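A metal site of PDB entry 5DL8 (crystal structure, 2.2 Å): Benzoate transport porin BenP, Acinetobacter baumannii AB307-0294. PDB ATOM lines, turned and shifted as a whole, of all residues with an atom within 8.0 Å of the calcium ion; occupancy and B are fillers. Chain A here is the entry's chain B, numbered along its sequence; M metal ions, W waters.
Water W1 bridges the side-chain carboxylate of Asp 42 (3.1 Å) and the backbone carbonyl oxygen of Asp 40 (3.4 Å).
N of Asp 38 is in hydrogen-bond range of O of Gly 395 (2.9 Å).
The calcium ion is bound by water W1, water W4, the side-chain carboxylate (OD1) of Asp 46, water W2, the side-chain carboxylate (OD1) of Asp 38, water W3, the backbone carbonyl oxygen (O) of Phe 39 and the side-chain carboxylate (OD2) of Asp 46.
The calcium ion has eight donor atoms within binding distance.
Within 4 Å of the calcium ion: Asp 38, Phe 39 and Asp 46.
Along chain A the residues within 4 Å of the calcium ion span positions 38 to 46.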
ATOM      1  N   ASN A  36      -8.363 -15.752 -11.236  1.00  0.00           N
ATOM      2  CA  ASN A  36      -8.078 -15.900  -9.806  1.00  0.00           C
ATOM      3  C   ASN A  36      -9.011 -16.907  -9.203  1.00  0.00           C
ATOM      4  O   ASN A  36     -10.220 -16.670  -9.123  1.00  0.00           O
ATOM      5  CB  ASN A  36      -8.151 -14.522  -9.016  1.00  0.00           C
ATOM      6  CG  ASN A  36      -7.401 -14.560  -7.708  1.00  0.00           C
ATOM      7  OD1 ASN A  36      -6.150 -14.590  -7.682  1.00  0.00           O
ATOM      8  ND2 ASN A  36      -8.125 -14.572  -6.637  1.00  0.00           N
ATOM      9  N   ARG A  37      -8.471 -18.046  -8.781  1.00  0.00           N
ATOM     10  CA  ARG A  37      -9.270 -19.015  -8.008  1.00  0.00           C
ATOM     11  C   ARG A  37      -8.910 -18.950  -6.546  1.00  0.00           C
ATOM     12  O   ARG A  37      -7.831 -19.289  -6.158  1.00  0.00           O
ATOM     13  CB  ARG A  37      -9.107 -20.462  -8.560  1.00  0.00           C
ATOM     14  CG  ARG A  37      -9.923 -21.549  -7.807  1.00  0.00           C
ATOM     15  CD  ARG A  37      -9.964 -22.909  -8.548  1.00  0.00           C
ATOM     16  NE  ARG A  37     -10.657 -22.859  -9.788  1.00  0.00           N
ATOM     17  CZ  ARG A  37     -10.970 -23.916 -10.584  1.00  0.00           C
ATOM     18  NH1 ARG A  37     -10.615 -25.154 -10.282  1.00  0.00           N
ATOM     19  NH2 ARG A  37     -11.661 -23.687 -11.742  1.00  0.00           N
ATOM     20  N   ASP A  38      -9.890 -18.644  -5.730  1.00  0.00           N
ATOM     21  CA  ASP A  38      -9.699 -18.425  -4.297  1.00  0.00           C
ATOM     22  C   ASP A  38     -10.457 -19.473  -3.511  1.00  0.00           C
ATOM     23  O   ASP A  38     -11.712 -19.420  -3.423  1.00  0.00           O
ATOM     24  CB  ASP A  38     -10.263 -16.998  -3.945  1.00  0.00           C
ATOM     25  CG  ASP A  38     -10.152 -16.641  -2.444  1.00  0.00           C
ATOM     26  OD1 ASP A  38     -10.116 -17.557  -1.599  1.00  0.00           O
ATOM     27  OD2 ASP A  38     -10.144 -15.439  -2.094  1.00  0.00           O
ATOM     28  N   PHE A  39      -9.734 -20.401  -2.901  1.00  0.00           N
ATOM     29  CA  PHE A  39     -10.323 -21.354  -1.924  1.00  0.00           C
ATOM     30  C   PHE A  39     -10.848 -20.705  -0.633  1.00  0.00           C
ATOM     31  O   PHE A  39     -10.210 -19.914  -0.041  1.00  0.00           O
ATOM     32  CB  PHE A  39      -9.377 -22.526  -1.705  1.00  0.00           C
ATOM     33  CG  PHE A  39      -9.049 -23.236  -2.995  1.00  0.00           C
ATOM     34  CD1 PHE A  39      -9.907 -24.232  -3.530  1.00  0.00           C
ATOM     35  CD2 PHE A  39      -7.929 -22.983  -3.684  1.00  0.00           C
ATOM     36  CE1 PHE A  39      -9.593 -24.894  -4.725  1.00  0.00           C
ATOM     37  CE2 PHE A  39      -7.576 -23.658  -4.843  1.00  0.00           C
ATOM     38  CZ  PHE A  39      -8.433 -24.584  -5.402  1.00  0.00           C
ATOM     39  N   ASP A  40     -12.092 -21.020  -0.237  1.00  0.00           N
ATOM     40  CA  ASP A  40     -12.623 -20.602   1.051  1.00  0.00           C
ATOM     41  C   ASP A  40     -11.715 -21.051   2.232  1.00  0.00           C
ATOM     42  O   ASP A  40     -11.449 -20.302   3.174  1.00  0.00           O
ATOM     43  CB  ASP A  40     -14.023 -21.176   1.240  1.00  0.00           C
ATOM     44  CG  ASP A  40     -15.064 -20.528   0.352  1.00  0.00           C
ATOM     45  OD1 ASP A  40     -14.796 -20.005  -0.720  1.00  0.00           O
ATOM     46  OD2 ASP A  40     -16.199 -20.546   0.696  1.00  0.00           O
ATOM     47  N   ASN A  41     -11.263 -22.296   2.185  1.00  0.00           N
ATOM     48  CA  ASN A  41     -10.388 -22.819   3.219  1.00  0.00           C
ATOM     49  C   ASN A  41      -8.943 -22.177   3.172  1.00  0.00           C
ATOM     50  O   ASN A  41      -8.181 -22.301   2.135  1.00  0.00           O
ATOM     51  CB  ASN A  41     -10.401 -24.326   3.098  1.00  0.00           C
ATOM     52  CG  ASN A  41      -9.516 -25.050   4.092  1.00  0.00           C
ATOM     53  OD1 ASN A  41      -8.869 -24.493   4.968  1.00  0.00           O
ATOM     54  ND2 ASN A  41      -9.520 -26.358   3.952  1.00  0.00           N
ATOM     55  N   ASP A  42      -8.590 -21.483   4.281  1.00  0.00           N
ATOM     56  CA  ASP A  42      -7.270 -20.788   4.474  1.00  0.00           C
ATOM     57  C   ASP A  42      -6.073 -21.713   4.330  1.00  0.00           C
ATOM     58  O   ASP A  42      -5.012 -21.220   3.965  1.00  0.00           O
ATOM     59  CB  ASP A  42      -7.162 -20.118   5.868  1.00  0.00           C
ATOM     60  CG  ASP A  42      -8.091 -18.949   6.030  1.00  0.00           C
ATOM     61  OD1 ASP A  42      -8.458 -18.341   5.038  1.00  0.00           O
ATOM     62  OD2 ASP A  42      -8.480 -18.619   7.146  1.00  0.00           O
ATOM     63  N   ALA A  43      -6.233 -23.018   4.655  1.00  0.00           N
ATOM     64  CA  ALA A  43      -5.166 -23.973   4.516  1.00  0.00           C
ATOM     65  C   ALA A  43      -4.752 -24.218   3.090  1.00  0.00           C
ATOM     66  O   ALA A  43      -3.680 -24.748   2.896  1.00  0.00           O
ATOM     67  CB  ALA A  43      -5.514 -25.278   5.160  1.00  0.00           C
ATOM     68  N   LEU A  44      -5.609 -23.897   2.102  1.00  0.00           N
ATOM     69  CA  LEU A  44      -5.263 -24.134   0.705  1.00  0.00           C
ATOM     70  C   LEU A  44      -4.713 -22.883   0.029  1.00  0.00           C
ATOM     71  O   LEU A  44      -5.086 -21.768   0.365  1.00  0.00           O
ATOM     72  CB  LEU A  44      -6.487 -24.684  -0.080  1.00  0.00           C
ATOM     73  CG  LEU A  44      -7.266 -25.886   0.520  1.00  0.00           C
ATOM     74  CD1 LEU A  44      -8.505 -26.220  -0.320  1.00  0.00           C
ATOM     75  CD2 LEU A  44      -6.417 -27.129   0.729  1.00  0.00           C
ATOM     76  N   LYS A  45      -3.910 -23.094  -1.007  1.00  0.00           N
ATOM     77  CA  LYS A  45      -3.353 -22.030  -1.795  1.00  0.00           C
ATOM     78  C   LYS A  45      -4.119 -21.588  -3.032  1.00  0.00           C
ATOM     79  O   LYS A  45      -4.378 -22.384  -3.958  1.00  0.00           O
ATOM     80  CB  LYS A  45      -1.954 -22.422  -2.250  1.00  0.00           C
ATOM     81  CG  LYS A  45      -1.016 -21.224  -2.537  1.00  0.00           C
ATOM     82  CD  LYS A  45       0.439 -21.646  -2.739  1.00  0.00           C
ATOM     83  CE  LYS A  45       0.836 -22.798  -1.799  1.00  0.00           C
ATOM     84  NZ  LYS A  45       2.278 -23.211  -1.869  1.00  0.00           N
ATOM     85  N   ASP A  46      -4.370 -20.279  -3.064  1.00  0.00           N
ATOM     86  CA  ASP A  46      -5.084 -19.581  -4.144  1.00  0.00           C
ATOM     87  C   ASP A  46      -4.278 -19.649  -5.445  1.00  0.00           C
ATOM     88  O   ASP A  46      -3.079 -19.627  -5.403  1.00  0.00           O
ATOM     89  CB  ASP A  46      -5.346 -18.145  -3.731  1.00  0.00           C
ATOM     90  CG  ASP A  46      -6.408 -18.034  -2.615  1.00  0.00           C
ATOM     91  OD1 ASP A  46      -7.102 -19.050  -2.163  1.00  0.00           O
ATOM     92  OD2 ASP A  46      -6.643 -16.875  -2.233  1.00  0.00           O
ATOM     93  N   THR A  47      -4.925 -19.865  -6.611  1.00  0.00           N
ATOM     94  CA  THR A  47      -4.178 -19.920  -7.842  1.00  0.00           C
ATOM     95  C   THR A  47      -4.670 -18.869  -8.815  1.00  0.00           C
ATOM     96  O   THR A  47      -5.745 -18.249  -8.657  1.00  0.00           O
ATOM     97  CB  THR A  47      -4.389 -21.287  -8.474  1.00  0.00           C
ATOM     98  OG1 THR A  47      -5.762 -21.394  -8.929  1.00  0.00           O
ATOM     99  CG2 THR A  47      -4.037 -22.412  -7.466  1.00  0.00           C
ATOM    100  N   ASP A 393     -14.404 -25.686  -1.259  1.00  0.00           N
ATOM    101  CA  ASP A 393     -15.240 -24.619  -1.820  1.00  0.00           C
ATOM    102  C   ASP A 393     -14.341 -23.554  -2.453  1.00  0.00           C
ATOM    103  O   ASP A 393     -13.229 -23.402  -1.977  1.00  0.00           O
ATOM    104  CB  ASP A 393     -16.088 -23.948  -0.776  1.00  0.00           C
ATOM    105  CG  ASP A 393     -17.098 -24.859  -0.172  1.00  0.00           C
ATOM    106  OD1 ASP A 393     -17.263 -25.990  -0.615  1.00  0.00           O
ATOM    107  OD2 ASP A 393     -17.771 -24.437   0.777  1.00  0.00           O
ATOM    108  N   PHE A 394     -14.765 -22.905  -3.560  1.00  0.00           N
ATOM    109  CA  PHE A 394     -14.020 -21.779  -4.064  1.00  0.00           C
ATOM    110  C   PHE A 394     -14.843 -20.692  -4.836  1.00  0.00           C
ATOM    111  O   PHE A 394     -15.967 -20.916  -5.297  1.00  0.00           O
ATOM    112  CB  PHE A 394     -12.864 -22.285  -4.904  1.00  0.00           C
ATOM    113  CG  PHE A 394     -13.280 -22.870  -6.237  1.00  0.00           C
ATOM    114  CD1 PHE A 394     -13.584 -22.045  -7.319  1.00  0.00           C
ATOM    115  CD2 PHE A 394     -13.283 -24.223  -6.422  1.00  0.00           C
ATOM    116  CE1 PHE A 394     -13.930 -22.563  -8.552  1.00  0.00           C
ATOM    117  CE2 PHE A 394     -13.642 -24.771  -7.651  1.00  0.00           C
ATOM    118  CZ  PHE A 394     -13.970 -23.935  -8.724  1.00  0.00           C
ATOM    119  N   GLY A 395     -14.236 -19.524  -4.946  1.00  0.00           N
ATOM    120  CA  GLY A 395     -14.718 -18.412  -5.798  1.00  0.00           C
ATOM    121  C   GLY A 395     -13.648 -18.032  -6.782  1.00  0.00           C
ATOM    122  O   GLY A 395     -12.533 -17.786  -6.397  1.00  0.00           O
HETATM  123 CA    CA M   1      -8.176 -18.259  -0.219  1.00  0.00          CA
HETATM  124  O   HOH W   1      -9.007 -18.333   1.948  1.00  0.00           O
HETATM  125  O   HOH W   2      -7.248 -20.321   0.535  1.00  0.00           O
HETATM  126  O   HOH W   3      -6.150 -17.757   1.209  1.00  0.00           O
HETATM  127  O   HOH W   4      -8.936 -16.189   0.538  1.00  0.00           O
